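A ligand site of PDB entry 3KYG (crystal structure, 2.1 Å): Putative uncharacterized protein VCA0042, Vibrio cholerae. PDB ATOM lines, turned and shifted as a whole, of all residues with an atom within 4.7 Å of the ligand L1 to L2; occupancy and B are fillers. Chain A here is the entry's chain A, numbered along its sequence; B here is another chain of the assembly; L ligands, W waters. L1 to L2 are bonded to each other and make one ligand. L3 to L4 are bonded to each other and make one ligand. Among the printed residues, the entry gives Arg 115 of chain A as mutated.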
ATOM      1  N   MET A  15      19.509  39.458  -2.359  1.00  0.00           N
ATOM      2  CA  MET A  15      19.637  37.994  -2.214  1.00  0.00           C
ATOM      3  C   MET A  15      18.544  37.430  -1.338  1.00  0.00           C
ATOM      4  O   MET A  15      18.371  36.196  -1.241  1.00  0.00           O
ATOM      5  CB  MET A  15      20.947  37.610  -1.518  1.00  0.00           C
ATOM      6  CG  MET A  15      22.186  38.165  -2.130  1.00  0.00           C
ATOM      7  SD  MET A  15      23.646  37.608  -1.155  1.00  0.00           S
ATOM      8  CE  MET A  15      24.887  38.532  -2.050  1.00  0.00           C
ATOM      9  N   ARG A  79      19.441  30.923  -2.406  1.00  0.00           N
ATOM     10  CA  ARG A  79      20.198  30.757  -3.643  1.00  0.00           C
ATOM     11  C   ARG A  79      21.343  29.752  -3.519  1.00  0.00           C
ATOM     12  O   ARG A  79      22.106  29.786  -2.545  1.00  0.00           O
ATOM     13  CB  ARG A  79      20.750  32.098  -4.114  1.00  0.00           C
ATOM     14  CG  ARG A  79      19.643  33.088  -4.374  1.00  0.00           C
ATOM     15  CD  ARG A  79      20.160  34.263  -5.159  1.00  0.00           C
ATOM     16  NE  ARG A  79      19.106  35.256  -5.335  1.00  0.00           N
ATOM     17  CZ  ARG A  79      19.308  36.505  -5.734  1.00  0.00           C
ATOM     18  NH1 ARG A  79      18.282  37.327  -5.851  1.00  0.00           N
ATOM     19  NH2 ARG A  79      20.541  36.927  -6.029  1.00  0.00           N
ATOM     20  N   GLY A  80      21.454  28.867  -4.508  1.00  0.00           N
ATOM     21  CA  GLY A  80      22.502  27.869  -4.505  1.00  0.00           C
ATOM     22  C   GLY A  80      22.444  27.021  -3.254  1.00  0.00           C
ATOM     23  O   GLY A  80      21.395  26.448  -2.960  1.00  0.00           O
ATOM     24  N   GLU A  81      23.556  26.943  -2.537  1.00  0.00           N
ATOM     25  CA  GLU A  81      23.598  26.140  -1.312  1.00  0.00           C
ATOM     26  C   GLU A  81      23.051  26.972  -0.169  1.00  0.00           C
ATOM     27  O   GLU A  81      22.956  26.498   0.964  1.00  0.00           O
ATOM     28  CB  GLU A  81      25.036  25.724  -0.983  1.00  0.00           C
ATOM     29  CG  GLU A  81      25.767  24.900  -2.055  1.00  0.00           C
ATOM     30  CD  GLU A  81      25.044  23.611  -2.405  1.00  0.00           C
ATOM     31  OE1 GLU A  81      24.515  22.963  -1.471  1.00  0.00           O
ATOM     32  OE2 GLU A  81      25.006  23.239  -3.603  1.00  0.00           O
ATOM     33  N   GLN A 114      28.552  33.118   2.310  1.00  0.00           N
ATOM     34  CA  GLN A 114      28.107  32.384   1.127  1.00  0.00           C
ATOM     35  C   GLN A 114      29.184  31.374   0.676  1.00  0.00           C
ATOM     36  O   GLN A 114      30.335  31.469   1.110  1.00  0.00           O
ATOM     37  CB  GLN A 114      27.856  33.372   0.010  1.00  0.00           C
ATOM     38  CG  GLN A 114      29.059  34.274  -0.253  1.00  0.00           C
ATOM     39  CD  GLN A 114      28.798  35.288  -1.345  1.00  0.00           C
ATOM     40  OE1 GLN A 114      28.423  34.933  -2.460  1.00  0.00           O
ATOM     41  NE2 GLN A 114      29.004  36.567  -1.031  1.00  0.00           N
ATOM     42  N   ARG A 115      28.813  30.440  -0.203  1.00  0.00           N
ATOM     43  CA  ARG A 115      29.791  29.430  -0.649  1.00  0.00           C
ATOM     44  C   ARG A 115      30.828  29.984  -1.615  1.00  0.00           C
ATOM     45  O   ARG A 115      31.954  29.500  -1.631  1.00  0.00           O
ATOM     46  CB  ARG A 115      29.095  28.227  -1.303  1.00  0.00           C
ATOM     47  CG  ARG A 115      28.366  27.275  -0.339  1.00  0.00           C
ATOM     48  CD  ARG A 115      29.293  26.685   0.704  1.00  0.00           C
ATOM     49  NE  ARG A 115      30.446  25.987   0.131  1.00  0.00           N
ATOM     50  CZ  ARG A 115      30.393  24.860  -0.572  1.00  0.00           C
ATOM     51  NH1 ARG A 115      29.214  24.270  -0.804  1.00  0.00           N
ATOM     52  NH2 ARG A 115      31.517  24.302  -1.032  1.00  0.00           N
ATOM     53  N   ARG A 116      30.466  30.980  -2.430  1.00  0.00           N
ATOM     54  CA  ARG A 116      31.425  31.564  -3.374  1.00  0.00           C
ATOM     55  C   ARG A 116      32.445  32.364  -2.590  1.00  0.00           C
ATOM     56  O   ARG A 116      32.082  33.231  -1.808  1.00  0.00           O
ATOM     57  CB  ARG A 116      30.728  32.467  -4.407  1.00  0.00           C
ATOM     58  CG  ARG A 116      29.901  31.695  -5.414  1.00  0.00           C
ATOM     59  CD  ARG A 116      29.262  32.546  -6.518  1.00  0.00           C
ATOM     60  NE  ARG A 116      28.305  31.725  -7.260  1.00  0.00           N
ATOM     61  CZ  ARG A 116      27.486  32.148  -8.224  1.00  0.00           C
ATOM     62  NH1 ARG A 116      26.668  31.302  -8.813  1.00  0.00           N
ATOM     63  NH2 ARG A 116      27.510  33.405  -8.602  1.00  0.00           N
ATOM     64  N   ARG A 120      31.928  37.261  -9.000  1.00  0.00           N
ATOM     65  CA  ARG A 120      32.038  36.894 -10.402  1.00  0.00           C
ATOM     66  C   ARG A 120      31.476  38.086 -11.145  1.00  0.00           C
ATOM     67  O   ARG A 120      30.405  38.574 -10.813  1.00  0.00           O
ATOM     68  CB  ARG A 120      31.215  35.652 -10.704  1.00  0.00           C
ATOM     69  CG  ARG A 120      31.606  34.471  -9.847  1.00  0.00           C
ATOM     70  CD  ARG A 120      30.834  33.232 -10.198  1.00  0.00           C
ATOM     71  NE  ARG A 120      31.252  32.120  -9.357  1.00  0.00           N
ATOM     72  CZ  ARG A 120      30.700  30.916  -9.388  1.00  0.00           C
ATOM     73  NH1 ARG A 120      29.713  30.677 -10.238  1.00  0.00           N
ATOM     74  NH2 ARG A 120      31.118  29.962  -8.556  1.00  0.00           N
ATOM     75  N   ARG A 149      32.107  31.557 -16.385  1.00  0.00           N
ATOM     76  CA  ARG A 149      30.903  30.893 -16.880  1.00  0.00           C
ATOM     77  C   ARG A 149      30.855  31.188 -18.368  1.00  0.00           C
ATOM     78  O   ARG A 149      31.094  32.322 -18.798  1.00  0.00           O
ATOM     79  CB  ARG A 149      29.647  31.461 -16.192  1.00  0.00           C
ATOM     80  CG  ARG A 149      28.274  31.029 -16.794  1.00  0.00           C
ATOM     81  CD  ARG A 149      27.204  31.019 -15.671  1.00  0.00           C
ATOM     82  NE  ARG A 149      27.665  30.083 -14.667  1.00  0.00           N
ATOM     83  CZ  ARG A 149      27.278  28.810 -14.571  1.00  0.00           C
ATOM     84  NH1 ARG A 149      26.351  28.336 -15.419  1.00  0.00           N
ATOM     85  NH2 ARG A 149      27.942  27.980 -13.758  1.00  0.00           N
ATOM     86  N   CYS A 187      33.769  22.432 -14.229  1.00  0.00           N
ATOM     87  CA  CYS A 187      33.332  22.130 -12.866  1.00  0.00           C
ATOM     88  C   CYS A 187      31.838  21.771 -12.838  1.00  0.00           C
ATOM     89  O   CYS A 187      31.404  20.877 -12.107  1.00  0.00           O
ATOM     90  CB  CYS A 187      33.577  23.338 -11.967  1.00  0.00           C
ATOM     91  SG  CYS A 187      32.692  23.273 -10.411  1.00  0.00           S
ATOM     92  N   ASN A 188      31.045  22.481 -13.633  1.00  0.00           N
ATOM     93  CA  ASN A 188      29.621  22.203 -13.691  1.00  0.00           C
ATOM     94  C   ASN A 188      29.047  22.548 -15.049  1.00  0.00           C
ATOM     95  O   ASN A 188      29.659  23.265 -15.828  1.00  0.00           O
ATOM     96  CB  ASN A 188      28.871  22.949 -12.565  1.00  0.00           C
ATOM     97  CG  ASN A 188      29.039  24.452 -12.619  1.00  0.00           C
ATOM     98  OD1 ASN A 188      28.314  25.146 -13.332  1.00  0.00           O
ATOM     99  ND2 ASN A 188      30.021  24.969 -11.870  1.00  0.00           N
ATOM    100  N   GLN A 190      25.047  22.866 -17.368  1.00  0.00           N
ATOM    101  CA  GLN A 190      23.589  22.790 -17.420  1.00  0.00           C
ATOM    102  C   GLN A 190      23.276  22.781 -18.909  1.00  0.00           C
ATOM    103  O   GLN A 190      23.633  23.706 -19.617  1.00  0.00           O
ATOM    104  CB  GLN A 190      22.967  24.003 -16.734  1.00  0.00           C
ATOM    105  CG  GLN A 190      23.410  24.154 -15.257  1.00  0.00           C
ATOM    106  CD  GLN A 190      24.775  24.837 -15.158  1.00  0.00           C
ATOM    107  OE1 GLN A 190      25.025  25.816 -15.840  1.00  0.00           O
ATOM    108  NE2 GLN A 190      25.648  24.334 -14.276  1.00  0.00           N
ATOM    109  N   SER B 192      27.598  18.202 -11.868  1.00  0.00           N
ATOM    110  CA  SER B 192      28.886  18.603 -11.315  1.00  0.00           C
ATOM    111  C   SER B 192      29.409  17.345 -10.638  1.00  0.00           C
ATOM    112  O   SER B 192      28.801  16.267 -10.758  1.00  0.00           O
ATOM    113  CB  SER B 192      28.752  19.710 -10.268  1.00  0.00           C
ATOM    114  OG  SER B 192      28.026  19.222  -9.153  1.00  0.00           O
ATOM    115  N   HIS B 195      26.503  16.970  -7.801  1.00  0.00           N
ATOM    116  CA  HIS B 195      25.059  16.963  -8.029  1.00  0.00           C
ATOM    117  C   HIS B 195      24.798  16.426  -9.420  1.00  0.00           C
ATOM    118  O   HIS B 195      25.647  16.547 -10.306  1.00  0.00           O
ATOM    119  CB  HIS B 195      24.494  18.378  -7.938  1.00  0.00           C
ATOM    120  CG  HIS B 195      25.054  19.159  -6.794  1.00  0.00           C
ATOM    121  ND1 HIS B 195      24.820  18.818  -5.479  1.00  0.00           N
ATOM    122  CD2 HIS B 195      25.934  20.190  -6.767  1.00  0.00           C
ATOM    123  CE1 HIS B 195      25.529  19.600  -4.685  1.00  0.00           C
ATOM    124  NE2 HIS B 195      26.222  20.441  -5.444  1.00  0.00           N
ATOM    125  N   ARG B 197      21.203  16.361 -11.630  1.00  0.00           N
ATOM    126  CA  ARG B 197      19.751  16.516 -11.700  1.00  0.00           C
ATOM    127  C   ARG B 197      19.288  16.424 -13.138  1.00  0.00           C
ATOM    128  O   ARG B 197      20.005  16.814 -14.061  1.00  0.00           O
ATOM    129  CB  ARG B 197      19.363  17.877 -11.106  1.00  0.00           C
ATOM    130  CG  ARG B 197      20.215  18.269  -9.917  1.00  0.00           C
ATOM    131  CD  ARG B 197      19.467  19.169  -8.962  1.00  0.00           C
ATOM    132  NE  ARG B 197      20.279  19.544  -7.812  1.00  0.00           N
ATOM    133  CZ  ARG B 197      21.158  20.540  -7.809  1.00  0.00           C
ATOM    134  NH1 ARG B 197      21.337  21.261  -8.905  1.00  0.00           N
ATOM    135  NH2 ARG B 197      21.866  20.817  -6.716  1.00  0.00           N
HETATM  136  P1  LIG L   1      24.200  31.354 -11.756  1.00  0.00           P
HETATM  137  O1  LIG L   1      23.907  31.800 -13.142  1.00  0.00           O
HETATM  138  O2  LIG L   1      25.474  31.943 -11.257  1.00  0.00           O
HETATM  139  O3  LIG L   1      24.397  29.768 -11.685  1.00  0.00           O
HETATM  140  C1  LIG L   1      23.448  28.938 -12.371  1.00  0.00           C
HETATM  141  C2  LIG L   1      23.687  27.463 -12.024  1.00  0.00           C
HETATM  142  O4  LIG L   1      25.009  27.044 -12.413  1.00  0.00           O
HETATM  143  C3  LIG L   1      23.633  27.273 -10.508  1.00  0.00           C
HETATM  144  O5  LIG L   1      22.265  27.148 -10.116  1.00  0.00           O
HETATM  145  C4  LIG L   1      24.310  25.902 -10.447  1.00  0.00           C
HETATM  146  O6  LIG L   1      23.434  24.893 -10.954  1.00  0.00           O
HETATM  147  C5  LIG L   1      25.469  26.109 -11.426  1.00  0.00           C
HETATM  148  N1  LIG L   1      26.640  26.716 -10.758  1.00  0.00           N
HETATM  149  C6  LIG L   1      27.016  27.991 -10.801  1.00  0.00           C
HETATM  150  N2  LIG L   1      28.163  28.129 -10.132  1.00  0.00           N
HETATM  151  C7  LIG L   1      28.514  26.935  -9.656  1.00  0.00           C
HETATM  152  C8  LIG L   1      29.619  26.457  -8.965  1.00  0.00           C
HETATM  153  O7  LIG L   1      30.500  27.230  -8.574  1.00  0.00           O
HETATM  154  N3  LIG L   1      29.713  25.094  -8.692  1.00  0.00           N
HETATM  155  C9  LIG L   1      28.685  24.243  -9.108  1.00  0.00           C
HETATM  156  N4  LIG L   1      28.734  22.938  -8.829  1.00  0.00           N
HETATM  157  N5  LIG L   1      27.631  24.727  -9.767  1.00  0.00           N
HETATM  158  C10 LIG L   1      27.536  26.034 -10.054  1.00  0.00           C
HETATM  159  P1  LG2 L   2      21.852  27.376  -8.577  1.00  0.00           P
HETATM  160  O1  LG2 L   2      22.685  26.584  -7.637  1.00  0.00           O
HETATM  161  O2  LG2 L   2      20.411  27.135  -8.354  1.00  0.00           O
HETATM  162  O3  LG2 L   2      22.073  28.942  -8.353  1.00  0.00           O
HETATM  163  C1  LG2 L   2      21.204  29.875  -8.993  1.00  0.00           C
HETATM  164  C2  LG2 L   2      21.725  31.292  -8.770  1.00  0.00           C
HETATM  165  O4  LG2 L   2      21.903  31.558  -7.371  1.00  0.00           O
HETATM  166  C3  LG2 L   2      23.127  31.405  -9.350  1.00  0.00           C
HETATM  167  O5  LG2 L   2      22.999  31.654 -10.755  1.00  0.00           O
HETATM  168  C4  LG2 L   2      23.585  32.669  -8.640  1.00  0.00           C
HETATM  169  O6  LG2 L   2      22.983  33.825  -9.231  1.00  0.00           O
HETATM  170  C5  LG2 L   2      23.021  32.460  -7.236  1.00  0.00           C
HETATM  171  N1  LG2 L   2      24.026  31.826  -6.350  1.00  0.00           N
HETATM  172  C6  LG2 L   2      24.187  30.527  -6.124  1.00  0.00           C
HETATM  173  N2  LG2 L   2      25.156  30.359  -5.218  1.00  0.00           N
HETATM  174  C7  LG2 L   2      25.610  31.566  -4.869  1.00  0.00           C
HETATM  175  C8  LG2 L   2      26.602  32.005  -3.998  1.00  0.00           C
HETATM  176  O7  LG2 L   2      27.230  31.205  -3.302  1.00  0.00           O
HETATM  177  N3  LG2 L   2      26.843  33.372  -3.878  1.00  0.00           N
HETATM  178  C9  LG2 L   2      26.086  34.265  -4.648  1.00  0.00           C
HETATM  179  N4  LG2 L   2      26.319  35.576  -4.553  1.00  0.00           N
HETATM  180  N5  LG2 L   2      25.132  33.814  -5.476  1.00  0.00           N
HETATM  181  C10 LG2 L   2      24.889  32.504  -5.598  1.00  0.00           C
HETATM  182  P1  LG3 L   3      32.914  24.019  -7.080  1.00  0.00           P
HETATM  183  O1  LG3 L   3      31.639  23.633  -7.742  1.00  0.00           O
HETATM  184  O2  LG3 L   3      33.871  22.896  -7.009  1.00  0.00           O
HETATM  185  O3  LG3 L   3      33.639  25.171  -7.918  1.00  0.00           O
HETATM  186  C1  LG3 L   3      34.958  25.610  -7.562  1.00  0.00           C
HETATM  187  C2  LG3 L   3      35.304  26.934  -8.266  1.00  0.00           C
HETATM  188  O4  LG3 L   3      35.156  26.867  -9.691  1.00  0.00           O
HETATM  189  C3  LG3 L   3      34.371  28.068  -7.862  1.00  0.00           C
HETATM  190  O5  LG3 L   3      34.736  28.518  -6.557  1.00  0.00           O
HETATM  191  C4  LG3 L   3      34.800  29.089  -8.911  1.00  0.00           C
HETATM  192  O6  LG3 L   3      36.091  29.618  -8.584  1.00  0.00           O
HETATM  193  C5  LG3 L   3      34.924  28.207 -10.161  1.00  0.00           C
HETATM  194  N1  LG3 L   3      33.649  28.240 -10.900  1.00  0.00           N
HETATM  195  C6  LG3 L   3      32.814  27.219 -11.098  1.00  0.00           C
HETATM  196  N2  LG3 L   3      31.795  27.635 -11.843  1.00  0.00           N
HETATM  197  C7  LG3 L   3      31.968  28.923 -12.123  1.00  0.00           C
HETATM  198  C8  LG3 L   3      31.240  29.859 -12.829  1.00  0.00           C
HETATM  199  O7  LG3 L   3      30.178  29.549 -13.383  1.00  0.00           O
HETATM  200  N3  LG3 L   3      31.717  31.166 -12.916  1.00  0.00           N
HETATM  201  C9  LG3 L   3      32.923  31.501 -12.287  1.00  0.00           C
HETATM  202  N4  LG3 L   3      33.386  32.747 -12.342  1.00  0.00           N
HETATM  203  N5  LG3 L   3      33.612  30.568 -11.614  1.00  0.00           N
HETATM  204  C10 LG3 L   3      33.162  29.307 -11.514  1.00  0.00           C
HETATM  205  P1  LG4 L   4      33.734  29.407  -5.681  1.00  0.00           P
HETATM  206  O1  LG4 L   4      33.065  30.437  -6.502  1.00  0.00           O
HETATM  207  O2  LG4 L   4      34.418  29.975  -4.497  1.00  0.00           O
HETATM  208  O3  LG4 L   4      32.654  28.355  -5.120  1.00  0.00           O
HETATM  209  C1  LG4 L   4      33.033  27.326  -4.209  1.00  0.00           C
HETATM  210  C2  LG4 L   4      31.897  26.314  -4.100  1.00  0.00           C
HETATM  211  O4  LG4 L   4      30.646  26.971  -3.807  1.00  0.00           O
HETATM  212  C3  LG4 L   4      31.666  25.673  -5.463  1.00  0.00           C
HETATM  213  O5  LG4 L   4      32.643  24.646  -5.638  1.00  0.00           O
HETATM  214  C4  LG4 L   4      30.286  25.060  -5.205  1.00  0.00           C
HETATM  215  O6  LG4 L   4      30.400  23.910  -4.366  1.00  0.00           O
HETATM  216  C5  LG4 L   4      29.602  26.194  -4.421  1.00  0.00           C
HETATM  217  N1  LG4 L   4      28.867  27.078  -5.361  1.00  0.00           N
HETATM  218  C6  LG4 L   4      29.286  28.224  -5.887  1.00  0.00           C
HETATM  219  N2  LG4 L   4      28.346  28.698  -6.698  1.00  0.00           N
HETATM  220  C7  LG4 L   4      27.315  27.858  -6.690  1.00  0.00           C
HETATM  221  C8  LG4 L   4      26.069  27.846  -7.306  1.00  0.00           C
HETATM  222  O7  LG4 L   4      25.732  28.744  -8.082  1.00  0.00           O
HETATM  223  N3  LG4 L   4      25.195  26.792  -7.040  1.00  0.00           N
HETATM  224  C9  LG4 L   4      25.592  25.774  -6.152  1.00  0.00           C
HETATM  225  N4  LG4 L   4      24.755  24.787  -5.838  1.00  0.00           N
HETATM  226  N5  LG4 L   4      26.794  25.818  -5.584  1.00  0.00           N
HETATM  227  C10 LG4 L   4      27.657  26.820  -5.829  1.00  0.00           C
HETATM  228  O   HOH W   1      24.010  31.740  -2.121  1.00  0.00           O
HETATM  229  O   HOH W   2      26.203  22.205  -9.794  1.00  0.00           O
HETATM  230  O   HOH W   3      26.154  29.943  -0.865  1.00  0.00           O
HETATM  231  O   HOH W   4      25.964  28.310  -3.282  1.00  0.00           O
HETATM  232  O   HOH W   5      19.270  28.378  -6.312  1.00  0.00           O
HETATM  233  O   HOH W   6      30.802  20.999  -7.425  1.00  0.00           O
HETATM  234  O   HOH W   7      28.047  32.111 -12.153  1.00  0.00           O
HETATM  235  O   HOH W   8      24.815  22.377 -12.060  1.00  0.00           O
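A nitrogen (N2) of LG3 L3 sits at hydrogen-bond distance from the side-chain amide nitrogen (ND2) of Asn 188.
The guanidinium group of Arg 120 sits at hydrogen-bond distance from an oxygen (O7) of LIG L1, at 2.8 Å.
The guanidinium group of Arg 149 lies close to an oxygen (O4) of LIG L1 (3.4 Å).
The side-chain carboxylate of Glu 81 sits at hydrogen-bond distance from a nitrogen (N4) of LG4 L4.
An oxygen (O1) of LG3 L3 sits at hydrogen-bond distance from the side-chain sulfur of Cys 187 (2.9 Å).
O2 of LIG L1 is in salt-bridge range of NH1 of Arg 116 (2.8 Å).
The guanidinium group of Arg 120 is in salt-bridge range of an oxygen (O1) of LG4 L4, 2.9 Å away.
The guanidinium group of Arg 149 is in hydrogen-bond range of an oxygen (O7) of LG3 L3 (2.8 Å).
OE1 of Gln 114 lies within hydrogen-bond range of N3 of LG2 L2, at 2.6 Å.
O7 of LG2 L2 sits at hydrogen-bond distance from N of Arg 116 (3.4 Å).
A nitrogen (N5) of LIG L1 lies close to the side-chain amide nitrogen (ND2) of Asn 188.
An oxygen (O7) of LG4 L4 lies within hydrogen-bond range of the guanidinium group (NH1) of Arg 116, 2.8 Å away.
The side-chain amide nitrogen (NE2) of Gln 190 sits at hydrogen-bond distance from an oxygen (O4) of LIG L1 (3.4 Å).
A nitrogen (N3) of LG4 L4 lies within hydrogen-bond range of an oxygen (O1) of LG2 L2 (2.6 Å).
The guanidinium group of Arg 149 sits at hydrogen-bond distance from the side-chain amide oxygen of Asn 188, 2.9 Å away.
OE1 of Gln 190 is in hydrogen-bond range of NH1 of Arg 149 (2.9 Å).
OG of Ser 192 of chain B is in hydrogen-bond range of N of His 195 of chain B (3.0 Å).
The side-chain amide oxygen (OD1) of Asn 188 lies within hydrogen-bond range of the side-chain amide nitrogen (NE2) of Gln 190, 2.9 Å away.
ND2 of Asn 188 sits at hydrogen-bond distance from SG of Cys 187, at 3.5 Å.
Residues that only touch the ligand L1 to L2: Gly 80 (3.4 Å), Arg 79 (3.5 Å), Ser 192 of chain B (3.5 Å), Arg 115 (3.6 Å) and Cys 187 (3.9 Å).
11 residues have an atom within 4 Å of the ligand L1 to L2: Arg 79, Gly 80, Gln 114, Arg 115, Arg 116, Arg 120, Arg 149, Cys 187, Asn 188, Gln 190 and Ser 192 of chain B.
The nearest printed residue that does not touch the ligand L1 to L2 is Met 15 (4.1 Å).
Water W5 bridges an oxygen (O2) of LG2 L2 and the backbone NH (N) of Gly 80.
Water W7 lies within hydrogen-bond range of O2 of LIG L1 (2.7 Å), NH1 of Arg 120 (2.9 Å) and NE of Arg 149 (3.3 Å).
Water W4 lies within hydrogen-bond range of the backbone NH (N) of Glu 81, a nitrogen (N2) of LG2 L2 and a nitrogen (N5) of LG4 L4.
Water W3 bridges N of Arg 115 (2.8 Å) and O7 of LG2 L2 (2.9 Å).
Water W8 bridges NE2 of Gln 190 (3.1 Å) and O6 of LIG L1 (3.1 Å).
Water W6 lies within hydrogen-bond range of O1 of LG3 L3 (2.8 Å) and N4 of LIG L1 (3.2 Å).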
